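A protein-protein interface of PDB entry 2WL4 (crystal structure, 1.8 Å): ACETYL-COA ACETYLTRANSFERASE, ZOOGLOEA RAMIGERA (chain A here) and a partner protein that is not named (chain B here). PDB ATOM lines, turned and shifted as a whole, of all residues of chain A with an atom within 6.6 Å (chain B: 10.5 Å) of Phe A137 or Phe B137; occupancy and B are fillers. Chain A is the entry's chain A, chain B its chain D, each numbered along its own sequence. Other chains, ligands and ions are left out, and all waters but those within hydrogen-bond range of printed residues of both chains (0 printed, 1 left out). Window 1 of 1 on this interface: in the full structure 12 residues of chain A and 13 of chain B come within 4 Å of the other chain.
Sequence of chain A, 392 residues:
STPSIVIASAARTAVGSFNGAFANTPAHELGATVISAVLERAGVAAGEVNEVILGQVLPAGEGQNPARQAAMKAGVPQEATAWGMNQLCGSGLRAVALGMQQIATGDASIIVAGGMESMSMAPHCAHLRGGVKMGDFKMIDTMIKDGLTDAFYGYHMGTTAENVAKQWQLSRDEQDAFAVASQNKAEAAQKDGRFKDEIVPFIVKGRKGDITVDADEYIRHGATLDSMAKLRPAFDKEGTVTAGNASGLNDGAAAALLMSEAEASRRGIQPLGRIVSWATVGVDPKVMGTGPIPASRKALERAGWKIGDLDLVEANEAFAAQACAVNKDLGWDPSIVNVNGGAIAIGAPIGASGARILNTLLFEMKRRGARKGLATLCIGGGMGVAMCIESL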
ATOM      1  N   HIS A 124      20.140 -21.758   7.660  1.00  0.00           N
ATOM      2  CA  HIS A 124      18.745 -21.886   7.284  1.00  0.00           C
ATOM      3  C   HIS A 124      18.161 -22.936   8.201  1.00  0.00           C
ATOM      4  O   HIS A 124      18.879 -23.813   8.664  1.00  0.00           O
ATOM      5  CB  HIS A 124      18.624 -22.346   5.829  1.00  0.00           C
ATOM      6  CG  HIS A 124      18.799 -21.243   4.832  1.00  0.00           C
ATOM      7  ND1 HIS A 124      20.011 -20.648   4.591  1.00  0.00           N
ATOM      8  CD2 HIS A 124      17.905 -20.650   4.004  1.00  0.00           C
ATOM      9  CE1 HIS A 124      19.861 -19.719   3.655  1.00  0.00           C
ATOM     10  NE2 HIS A 124      18.598 -19.701   3.288  1.00  0.00           N
ATOM     11  N   CYS A 125      16.868 -22.859   8.477  1.00  0.00           N
ATOM     12  CA  CYS A 125      16.312 -23.750   9.475  1.00  0.00           C
ATOM     13  C   CYS A 125      14.878 -24.169   9.181  1.00  0.00           C
ATOM     14  O   CYS A 125      14.211 -23.609   8.300  1.00  0.00           O
ATOM     15  CB  CYS A 125      16.419 -23.124  10.876  1.00  0.00           C
ATOM     16  SG  CYS A 125      15.238 -21.796  11.234  1.00  0.00           S
ATOM     17  N   ALA A 126      14.410 -25.172   9.910  1.00  0.00           N
ATOM     18  CA  ALA A 126      13.010 -25.559   9.827  1.00  0.00           C
ATOM     19  C   ALA A 126      12.629 -26.408  11.023  1.00  0.00           C
ATOM     20  O   ALA A 126      13.412 -27.228  11.470  1.00  0.00           O
ATOM     21  CB  ALA A 126      12.751 -26.339   8.554  1.00  0.00           C
ATOM     22  N   LEU A 128      11.088 -29.455  12.306  1.00  0.00           N
ATOM     23  CA  LEU A 128      10.808 -30.745  11.667  1.00  0.00           C
ATOM     24  C   LEU A 128      10.419 -31.863  12.642  1.00  0.00           C
ATOM     25  O   LEU A 128      10.370 -33.035  12.248  1.00  0.00           O
ATOM     26  CB  LEU A 128      12.023 -31.181  10.849  1.00  0.00           C
ATOM     27  CG  LEU A 128      12.367 -30.297   9.637  1.00  0.00           C
ATOM     28  CD1 LEU A 128      13.712 -30.658   9.049  1.00  0.00           C
ATOM     29  CD2 LEU A 128      11.279 -30.422   8.583  1.00  0.00           C
ATOM     30  N   VAL A 132       6.105 -33.483   8.132  1.00  0.00           N
ATOM     31  CA  VAL A 132       5.452 -33.094   6.888  1.00  0.00           C
ATOM     32  C   VAL A 132       5.576 -34.264   5.915  1.00  0.00           C
ATOM     33  O   VAL A 132       6.566 -34.385   5.195  1.00  0.00           O
ATOM     34  CB  VAL A 132       6.086 -31.828   6.271  1.00  0.00           C
ATOM     35  CG1 VAL A 132       5.083 -31.118   5.383  1.00  0.00           C
ATOM     36  CG2 VAL A 132       6.583 -30.886   7.362  1.00  0.00           C
ATOM     37  N   GLY A 135       4.943 -33.262   0.174  1.00  0.00           N
ATOM     38  CA  GLY A 135       5.063 -31.903  -0.342  1.00  0.00           C
ATOM     39  C   GLY A 135       6.231 -31.079   0.219  1.00  0.00           C
ATOM     40  O   GLY A 135       6.805 -31.406   1.257  1.00  0.00           O
ATOM     41  N   ASP A 136       6.589 -30.002  -0.475  1.00  0.00           N
ATOM     42  CA  ASP A 136       7.725 -29.164  -0.074  1.00  0.00           C
ATOM     43  C   ASP A 136       7.479 -28.461   1.258  1.00  0.00           C
ATOM     44  O   ASP A 136       6.336 -28.277   1.666  1.00  0.00           O
ATOM     45  CB  ASP A 136       8.023 -28.091  -1.127  1.00  0.00           C
ATOM     46  CG  ASP A 136       7.885 -28.598  -2.546  1.00  0.00           C
ATOM     47  OD1 ASP A 136       8.282 -29.748  -2.814  1.00  0.00           O
ATOM     48  OD2 ASP A 136       7.392 -27.834  -3.403  1.00  0.00           O
ATOM     49  N   PHE A 137       8.560 -28.054   1.917  1.00  0.00           N
ATOM     50  CA  PHE A 137       8.461 -27.179   3.087  1.00  0.00           C
ATOM     51  C   PHE A 137       9.507 -26.057   2.979  1.00  0.00           C
ATOM     52  O   PHE A 137      10.446 -26.160   2.191  1.00  0.00           O
ATOM     53  CB  PHE A 137       8.589 -27.966   4.406  1.00  0.00           C
ATOM     54  CG  PHE A 137       9.858 -28.764   4.521  1.00  0.00           C
ATOM     55  CD1 PHE A 137      11.014 -28.191   5.041  1.00  0.00           C
ATOM     56  CD2 PHE A 137       9.898 -30.086   4.110  1.00  0.00           C
ATOM     57  CE1 PHE A 137      12.184 -28.927   5.149  1.00  0.00           C
ATOM     58  CE2 PHE A 137      11.067 -30.825   4.206  1.00  0.00           C
ATOM     59  CZ  PHE A 137      12.211 -30.248   4.727  1.00  0.00           C
ATOM     60  N   LYS A 138       9.327 -24.994   3.749  1.00  0.00           N
ATOM     61  CA  LYS A 138      10.252 -23.854   3.726  1.00  0.00           C
ATOM     62  C   LYS A 138      11.463 -24.019   4.640  1.00  0.00           C
ATOM     63  O   LYS A 138      11.315 -24.253   5.843  1.00  0.00           O
ATOM     64  CB  LYS A 138       9.526 -22.577   4.147  1.00  0.00           C
ATOM     65  CG  LYS A 138       8.909 -21.784   3.021  1.00  0.00           C
ATOM     66  CD  LYS A 138       8.129 -20.593   3.564  1.00  0.00           C
ATOM     67  CE  LYS A 138       7.705 -19.658   2.442  1.00  0.00           C
ATOM     68  NZ  LYS A 138       6.596 -18.756   2.852  1.00  0.00           N
ATOM     69  N   MET A 139      12.655 -23.881   4.070  1.00  0.00           N
ATOM     70  CA  MET A 139      13.847 -23.659   4.873  1.00  0.00           C
ATOM     71  C   MET A 139      14.027 -22.149   5.014  1.00  0.00           C
ATOM     72  O   MET A 139      14.108 -21.425   4.014  1.00  0.00           O
ATOM     73  CB  MET A 139      15.077 -24.296   4.234  1.00  0.00           C
ATOM     74  CG  MET A 139      15.090 -25.818   4.314  1.00  0.00           C
ATOM     75  SD  MET A 139      15.490 -26.410   5.977  1.00  0.00           S
ATOM     76  CE  MET A 139      17.271 -26.263   5.932  1.00  0.00           C
ATOM     77  N   ILE A 140      14.079 -21.708   6.266  1.00  0.00           N
ATOM     78  CA  ILE A 140      14.000 -20.299   6.651  1.00  0.00           C
ATOM     79  C   ILE A 140      15.407 -19.749   6.902  1.00  0.00           C
ATOM     80  O   ILE A 140      16.159 -20.317   7.674  1.00  0.00           O
ATOM     81  CB  ILE A 140      13.123 -20.181   7.938  1.00  0.00           C
ATOM     82  CG1 ILE A 140      11.694 -20.679   7.639  1.00  0.00           C
ATOM     83  CG2 ILE A 140      13.130 -18.769   8.519  1.00  0.00           C
ATOM     84  CD1 ILE A 140      10.922 -19.751   6.711  1.00  0.00           C
ATOM     85  N   ASP A 141      15.758 -18.658   6.221  1.00  0.00           N
ATOM     86  CA  ASP A 141      17.026 -17.985   6.433  1.00  0.00           C
ATOM     87  C   ASP A 141      16.989 -17.302   7.822  1.00  0.00           C
ATOM     88  O   ASP A 141      16.270 -16.322   8.019  1.00  0.00           O
ATOM     89  CB  ASP A 141      17.268 -16.959   5.307  1.00  0.00           C
ATOM     90  CG  ASP A 141      18.660 -16.370   5.335  1.00  0.00           C
ATOM     91  OD1 ASP A 141      19.250 -16.316   6.444  1.00  0.00           O
ATOM     92  OD2 ASP A 141      19.164 -15.915   4.265  1.00  0.00           O
ATOM     93  N   ALA B 122      10.849 -42.225  -0.720  1.00  0.00           N
ATOM     94  CA  ALA B 122      11.324 -41.128  -1.552  1.00  0.00           C
ATOM     95  C   ALA B 122      11.583 -39.925  -0.651  1.00  0.00           C
ATOM     96  O   ALA B 122      10.710 -39.522   0.099  1.00  0.00           O
ATOM     97  CB  ALA B 122      10.298 -40.793  -2.600  1.00  0.00           C
ATOM     98  N   PRO B 123      12.791 -39.350  -0.732  1.00  0.00           N
ATOM     99  CA  PRO B 123      13.257 -38.320   0.195  1.00  0.00           C
ATOM    100  C   PRO B 123      12.861 -36.910  -0.244  1.00  0.00           C
ATOM    101  O   PRO B 123      12.256 -36.751  -1.304  1.00  0.00           O
ATOM    102  CB  PRO B 123      14.786 -38.474   0.133  1.00  0.00           C
ATOM    103  CG  PRO B 123      15.065 -39.543  -1.020  1.00  0.00           C
ATOM    104  CD  PRO B 123      13.796 -39.653  -1.766  1.00  0.00           C
ATOM    105  N   HIS B 124      13.199 -35.913   0.572  1.00  0.00           N
ATOM    106  CA  HIS B 124      13.156 -34.503   0.170  1.00  0.00           C
ATOM    107  C   HIS B 124      14.552 -34.049  -0.220  1.00  0.00           C
ATOM    108  O   HIS B 124      15.544 -34.603   0.262  1.00  0.00           O
ATOM    109  CB  HIS B 124      12.656 -33.632   1.313  1.00  0.00           C
ATOM    110  CG  HIS B 124      11.172 -33.695   1.523  1.00  0.00           C
ATOM    111  ND1 HIS B 124      10.520 -34.841   1.933  1.00  0.00           N
ATOM    112  CD2 HIS B 124      10.215 -32.747   1.392  1.00  0.00           C
ATOM    113  CE1 HIS B 124       9.228 -34.593   2.048  1.00  0.00           C
ATOM    114  NE2 HIS B 124       9.016 -33.327   1.732  1.00  0.00           N
ATOM    115  N   CYS B 125      14.649 -33.035  -1.076  1.00  0.00           N
ATOM    116  CA  CYS B 125      15.954 -32.635  -1.571  1.00  0.00           C
ATOM    117  C   CYS B 125      16.003 -31.195  -2.043  1.00  0.00           C
ATOM    118  O   CYS B 125      14.973 -30.526  -2.194  1.00  0.00           O
ATOM    119  CB  CYS B 125      16.371 -33.539  -2.733  1.00  0.00           C
ATOM    120  SG  CYS B 125      15.607 -33.083  -4.323  1.00  0.00           S
ATOM    121  N   ALA B 126      17.223 -30.742  -2.297  1.00  0.00           N
ATOM    122  CA  ALA B 126      17.460 -29.434  -2.859  1.00  0.00           C
ATOM    123  C   ALA B 126      18.854 -29.373  -3.438  1.00  0.00           C
ATOM    124  O   ALA B 126      19.759 -30.075  -2.979  1.00  0.00           O
ATOM    125  CB  ALA B 126      17.307 -28.364  -1.792  1.00  0.00           C
ATOM    126  N   HIS B 127      19.036 -28.516  -4.435  1.00  0.00           N
ATOM    127  CA  HIS B 127      20.362 -28.286  -4.965  1.00  0.00           C
ATOM    128  C   HIS B 127      21.056 -27.202  -4.149  1.00  0.00           C
ATOM    129  O   HIS B 127      20.633 -26.050  -4.157  1.00  0.00           O
ATOM    130  CB  HIS B 127      20.308 -27.912  -6.445  1.00  0.00           C
ATOM    131  CG  HIS B 127      21.658 -27.671  -7.044  1.00  0.00           C
ATOM    132  ND1 HIS B 127      22.048 -26.444  -7.530  1.00  0.00           N
ATOM    133  CD2 HIS B 127      22.720 -28.497  -7.204  1.00  0.00           C
ATOM    134  CE1 HIS B 127      23.289 -26.526  -7.981  1.00  0.00           C
ATOM    135  NE2 HIS B 127      23.718 -27.760  -7.792  1.00  0.00           N
ATOM    136  N   LEU B 128      22.133 -27.584  -3.464  1.00  0.00           N
ATOM    137  CA  LEU B 128      22.819 -26.708  -2.517  1.00  0.00           C
ATOM    138  C   LEU B 128      24.298 -26.610  -2.835  1.00  0.00           C
ATOM    139  O   LEU B 128      25.067 -25.969  -2.115  1.00  0.00           O
ATOM    140  CB  LEU B 128      22.629 -27.251  -1.095  1.00  0.00           C
ATOM    141  CG  LEU B 128      21.199 -27.691  -0.774  1.00  0.00           C
ATOM    142  CD1 LEU B 128      21.141 -28.419   0.568  1.00  0.00           C
ATOM    143  CD2 LEU B 128      20.242 -26.500  -0.801  1.00  0.00           C
ATOM    144  N   ARG B 129      24.696 -27.243  -3.931  1.00  0.00           N
ATOM    145  CA  ARG B 129      26.095 -27.267  -4.326  1.00  0.00           C
ATOM    146  C   ARG B 129      26.590 -25.856  -4.614  1.00  0.00           C
ATOM    147  O   ARG B 129      27.708 -25.490  -4.247  1.00  0.00           O
ATOM    148  CB  ARG B 129      26.274 -28.156  -5.556  1.00  0.00           C
ATOM    149  CG  ARG B 129      27.559 -28.947  -5.555  1.00  0.00           C
ATOM    150  CD  ARG B 129      27.600 -29.929  -6.719  1.00  0.00           C
ATOM    151  NE  ARG B 129      26.598 -30.985  -6.619  1.00  0.00           N
ATOM    152  CZ  ARG B 129      26.670 -32.017  -5.781  1.00  0.00           C
ATOM    153  NH1 ARG B 129      27.688 -32.126  -4.934  1.00  0.00           N
ATOM    154  NH2 ARG B 129      25.704 -32.932  -5.773  1.00  0.00           N
ATOM    155  N   GLY B 131      24.891 -23.255  -3.477  1.00  0.00           N
ATOM    156  CA  GLY B 131      24.566 -22.526  -2.267  1.00  0.00           C
ATOM    157  C   GLY B 131      23.252 -21.776  -2.350  1.00  0.00           C
ATOM    158  O   GLY B 131      22.599 -21.741  -3.397  1.00  0.00           O
ATOM    159  N   VAL B 132      22.863 -21.179  -1.231  1.00  0.00           N
ATOM    160  CA  VAL B 132      21.646 -20.387  -1.144  1.00  0.00           C
ATOM    161  C   VAL B 132      22.018 -19.092  -0.437  1.00  0.00           C
ATOM    162  O   VAL B 132      21.838 -18.958   0.773  1.00  0.00           O
ATOM    163  CB  VAL B 132      20.566 -21.139  -0.350  1.00  0.00           C
ATOM    164  CG1 VAL B 132      19.256 -20.360  -0.334  1.00  0.00           C
ATOM    165  CG2 VAL B 132      20.357 -22.527  -0.940  1.00  0.00           C
ATOM    166  N   LYS B 133      22.545 -18.147  -1.207  1.00  0.00           N
ATOM    167  CA  LYS B 133      23.187 -16.952  -0.663  1.00  0.00           C
ATOM    168  C   LYS B 133      22.396 -16.226   0.430  1.00  0.00           C
ATOM    169  O   LYS B 133      22.975 -15.777   1.411  1.00  0.00           O
ATOM    170  CB  LYS B 133      23.544 -15.986  -1.792  1.00  0.00           C
ATOM    171  CG  LYS B 133      24.554 -16.550  -2.780  1.00  0.00           C
ATOM    172  CD  LYS B 133      25.840 -16.951  -2.080  1.00  0.00           C
ATOM    173  CE  LYS B 133      26.814 -17.594  -3.050  1.00  0.00           C
ATOM    174  NZ  LYS B 133      26.208 -18.771  -3.723  1.00  0.00           N
ATOM    175  N   MET B 134      21.080 -16.125   0.260  1.00  0.00           N
ATOM    176  CA  MET B 134      20.234 -15.373   1.186  1.00  0.00           C
ATOM    177  C   MET B 134      18.755 -15.578   0.871  1.00  0.00           C
ATOM    178  O   MET B 134      18.369 -15.562  -0.293  1.00  0.00           O
ATOM    179  CB  MET B 134      20.576 -13.888   1.078  1.00  0.00           C
ATOM    180  CG  MET B 134      19.482 -12.934   1.506  1.00  0.00           C
ATOM    181  SD  MET B 134      20.025 -11.215   1.325  1.00  0.00           S
ATOM    182  CE  MET B 134      20.322 -11.137  -0.441  1.00  0.00           C
ATOM    183  N   GLY B 135      17.929 -15.752   1.901  1.00  0.00           N
ATOM    184  CA  GLY B 135      16.490 -15.870   1.719  1.00  0.00           C
ATOM    185  C   GLY B 135      15.978 -17.297   1.828  1.00  0.00           C
ATOM    186  O   GLY B 135      16.749 -18.247   1.744  1.00  0.00           O
ATOM    187  N   ASP B 136      14.680 -17.446   2.044  1.00  0.00           N
ATOM    188  CA  ASP B 136      14.102 -18.780   2.239  1.00  0.00           C
ATOM    189  C   ASP B 136      14.148 -19.596   0.942  1.00  0.00           C
ATOM    190  O   ASP B 136      14.233 -19.029  -0.148  1.00  0.00           O
ATOM    191  CB  ASP B 136      12.667 -18.657   2.717  1.00  0.00           C
ATOM    192  CG  ASP B 136      12.559 -17.926   4.013  1.00  0.00           C
ATOM    193  OD1 ASP B 136      13.619 -17.656   4.620  1.00  0.00           O
ATOM    194  OD2 ASP B 136      11.423 -17.612   4.415  1.00  0.00           O
ATOM    195  N   PHE B 137      14.101 -20.921   1.064  1.00  0.00           N
ATOM    196  CA  PHE B 137      14.041 -21.805  -0.107  1.00  0.00           C
ATOM    197  C   PHE B 137      13.207 -23.054   0.176  1.00  0.00           C
ATOM    198  O   PHE B 137      12.693 -23.220   1.289  1.00  0.00           O
ATOM    199  CB  PHE B 137      15.443 -22.190  -0.588  1.00  0.00           C
ATOM    200  CG  PHE B 137      16.130 -23.221   0.265  1.00  0.00           C
ATOM    201  CD1 PHE B 137      16.022 -24.574  -0.033  1.00  0.00           C
ATOM    202  CD2 PHE B 137      16.893 -22.843   1.353  1.00  0.00           C
ATOM    203  CE1 PHE B 137      16.658 -25.524   0.743  1.00  0.00           C
ATOM    204  CE2 PHE B 137      17.534 -23.784   2.132  1.00  0.00           C
ATOM    205  CZ  PHE B 137      17.413 -25.130   1.829  1.00  0.00           C
ATOM    206  N   LYS B 138      13.073 -23.923  -0.832  1.00  0.00           N
ATOM    207  CA  LYS B 138      12.296 -25.160  -0.696  1.00  0.00           C
ATOM    208  C   LYS B 138      13.135 -26.433  -0.716  1.00  0.00           C
ATOM    209  O   LYS B 138      14.052 -26.589  -1.525  1.00  0.00           O
ATOM    210  CB  LYS B 138      11.243 -25.266  -1.803  1.00  0.00           C
ATOM    211  CG  LYS B 138      10.198 -24.160  -1.821  1.00  0.00           C
ATOM    212  CD  LYS B 138       9.459 -24.162  -3.152  1.00  0.00           C
ATOM    213  CE  LYS B 138       8.583 -22.931  -3.315  1.00  0.00           C
ATOM    214  NZ  LYS B 138       7.877 -22.934  -4.629  1.00  0.00           N
ATOM    215  N   MET B 139      12.798 -27.350   0.182  1.00  0.00           N
ATOM    216  CA  MET B 139      13.184 -28.751   0.044  1.00  0.00           C
ATOM    217  C   MET B 139      11.990 -29.427  -0.678  1.00  0.00           C
ATOM    218  O   MET B 139      10.841 -29.336  -0.213  1.00  0.00           O
ATOM    219  CB  MET B 139      13.467 -29.353   1.446  1.00  0.00           C
ATOM    220  CG  MET B 139      14.711 -28.870   2.095  1.00  0.00           C
ATOM    221  SD  MET B 139      16.202 -29.690   1.464  1.00  0.00           S
ATOM    222  CE  MET B 139      15.991 -31.345   2.118  1.00  0.00           C
ATOM    223  N   ILE B 140      12.216 -30.049  -1.837  1.00  0.00           N
ATOM    224  CA  ILE B 140      11.052 -30.558  -2.644  1.00  0.00           C
ATOM    225  C   ILE B 140      10.158 -31.761  -2.154  1.00  0.00           C
ATOM    226  O   ILE B 140       9.248 -31.572  -1.341  1.00  0.00           O
ATOM    227  CB  ILE B 140      11.401 -30.686  -4.155  1.00  0.00           C
ATOM    228  CG1 ILE B 140      12.687 -31.474  -4.358  1.00  0.00           C
ATOM    229  CG2 ILE B 140      11.558 -29.304  -4.778  1.00  0.00           C
ATOM    230  CD1 ILE B 140      12.610 -32.885  -3.908  1.00  0.00           C
ATOM    231  N   ASP B 141      10.377 -32.962  -2.691  1.00  0.00           N
ATOM    232  CA  ASP B 141       9.596 -34.160  -2.326  1.00  0.00           C
ATOM    233  C   ASP B 141       9.890 -35.386  -3.211  1.00  0.00           C
ATOM    234  O   ASP B 141       9.541 -36.516  -2.860  1.00  0.00           O
ATOM    235  CB  ASP B 141       8.086 -33.861  -2.334  1.00  0.00           C
ATOM    236  CG  ASP B 141       7.240 -35.088  -2.037  1.00  0.00           C
ATOM    237  OD1 ASP B 141       7.125 -35.955  -2.924  1.00  0.00           O
ATOM    238  OD2 ASP B 141       6.672 -35.180  -0.925  1.00  0.00           O
ATOM    239  N   THR B 142      10.534 -35.153  -4.347  1.00  0.00           N
ATOM    240  CA  THR B 142      10.823 -36.186  -5.357  1.00  0.00           C
ATOM    241  C   THR B 142       9.632 -37.048  -5.788  1.00  0.00           C
ATOM    242  O   THR B 142       9.473 -37.339  -6.971  1.00  0.00           O
ATOM    243  CB  THR B 142      12.040 -37.085  -4.982  1.00  0.00           C
ATOM    244  OG1 THR B 142      11.660 -38.089  -4.030  1.00  0.00           O
ATOM    245  CG2 THR B 142      13.165 -36.241  -4.420  1.00  0.00           C
ATOM    246  N   ILE B 144       6.371 -36.133  -5.343  1.00  0.00           N
ATOM    247  CA  ILE B 144       5.499 -35.158  -5.968  1.00  0.00           C
ATOM    248  C   ILE B 144       6.176 -34.549  -7.196  1.00  0.00           C
ATOM    249  O   ILE B 144       5.643 -34.619  -8.295  1.00  0.00           O
ATOM    250  CB  ILE B 144       5.112 -34.036  -4.987  1.00  0.00           C
ATOM    251  CG1 ILE B 144       4.230 -34.585  -3.861  1.00  0.00           C
ATOM    252  CG2 ILE B 144       4.411 -32.893  -5.722  1.00  0.00           C
ATOM    253  CD1 ILE B 144       2.750 -34.427  -4.105  1.00  0.00           C
ATOM    254  N   LYS B 145       7.368 -33.988  -7.001  1.00  0.00           N
ATOM    255  CA  LYS B 145       8.076 -33.240  -8.045  1.00  0.00           C
ATOM    256  C   LYS B 145       8.576 -34.105  -9.187  1.00  0.00           C
ATOM    257  O   LYS B 145       8.612 -33.670 -10.344  1.00  0.00           O
ATOM    258  CB  LYS B 145       9.268 -32.488  -7.434  1.00  0.00           C
ATOM    259  CG  LYS B 145      10.350 -32.049  -8.431  1.00  0.00           C
ATOM    260  CD  LYS B 145       9.832 -30.988  -9.396  1.00  0.00           C
ATOM    261  CE  LYS B 145      10.895 -29.972  -9.738  1.00  0.00           C
ATOM    262  NZ  LYS B 145      10.357 -28.863 -10.585  1.00  0.00           N
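The backbone NH of Asp A136 lies close to the backbone carbonyl oxygen of Ile B140, 3.2 Å away.
OD2 of Asp B141 lies within hydrogen-bond range of N of Gly A135 (2.8 Å).
The backbone carbonyl oxygen of Phe A137 sits at hydrogen-bond distance from the backbone NH of Met B139 (3.3 Å).
The backbone NH (N) of Gly B135 sits at hydrogen-bond distance from the side-chain carboxylate (OD2) of Asp A141 (2.7 Å).
OD1 of Asp B136 sits at hydrogen-bond distance from N of Asp A141 (2.9 Å).
O of Gly B135 lies within hydrogen-bond range of NE2 of His A124, 2.8 Å away.
The backbone carbonyl oxygen (O) of Gly A135 is in hydrogen-bond range of a ring nitrogen (NE2) of His B124.
The backbone carbonyl oxygen of Phe B137 lies within hydrogen-bond range of the backbone NH of Met A139 (2.9 Å).
Printed residues of chain A that touch a printed residue of chain B: His A124, Gly A135, Asp A136, Phe A137, Lys A138, Met A139, Ile A140 and Asp A141.
Hydrophobic or aromatic side chains of chain A that line the printed part of chain B: His A124, Phe A137, Met A139 and Ile A140.
Of the 22 printed residues of chain B, 10 touch a printed residue of chain A.
Among the printed residues, no Asp or Glu carboxylate lies within 4 Å of a Lys or Arg side-chain nitrogen of the other chain.
Of chain B, only Met B139 (3.1 Å), Ile B140 (2.5 Å) and Asp B141 (3.8 Å) come within 4 Å of Asp A136.
Phe A137 touches four residues of chain B.
Printed residues of chain B within 4 Å of Asp A141: Met B134 (3.3 Å), Gly B135 (2.7 Å) and Asp B136 (2.9 Å).
Of the printed residues of chain A, Gly B135 touches His A124 (2.8 Å) and Asp A141 (2.7 Å).
Printed residues of chain A within 4 Å of Asp B136: Met A139, Ile A140 and Asp A141.
Phe B137 touches just these residues of chain A: His A124, Phe A137, Lys A138 and Met A139.
Printed residues of chain A within 4 Å of Lys B138: Phe A137.
Thr B142 touches none of the printed residues of chain A.
The nearest residue of chain A that does not touch Phe B137 is Ile A140 (5.3 Å).
The nearest printed residue of chain A that does not touch Val B132 is Asp A141 (5.3 Å).
O of Cys B125 is in hydrogen-bond range of N of Ile B140, at 2.8 Å.
The backbone carbonyl oxygen (O) of Ile A140 sits at hydrogen-bond distance from the backbone NH (N) of Cys A125.
OD1 of Asp B141 sits at hydrogen-bond distance from N of Ile B144, 2.5 Å away.
Val B132 touches His A124.
Gly A135 touches Ile B140.
O of Met B139 touches CA of Asp A136, 3.1 Å away.
Asp A136 touches Asp B141 (OD1 to N, 3.8 Å).
CE2 of Phe A137 touches CD2 of His B124, at 3.5 Å.
O of Phe A137 touches O of Phe B137 (3.8 Å).
Lys B138 touches Phe A137 (CA to O, 3.6 Å).
Met B139 touches Met A139.
Asp B136 touches Ile A140.
OD2 of Asp A141 touches CA of Met B134, 3.3 Å away.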
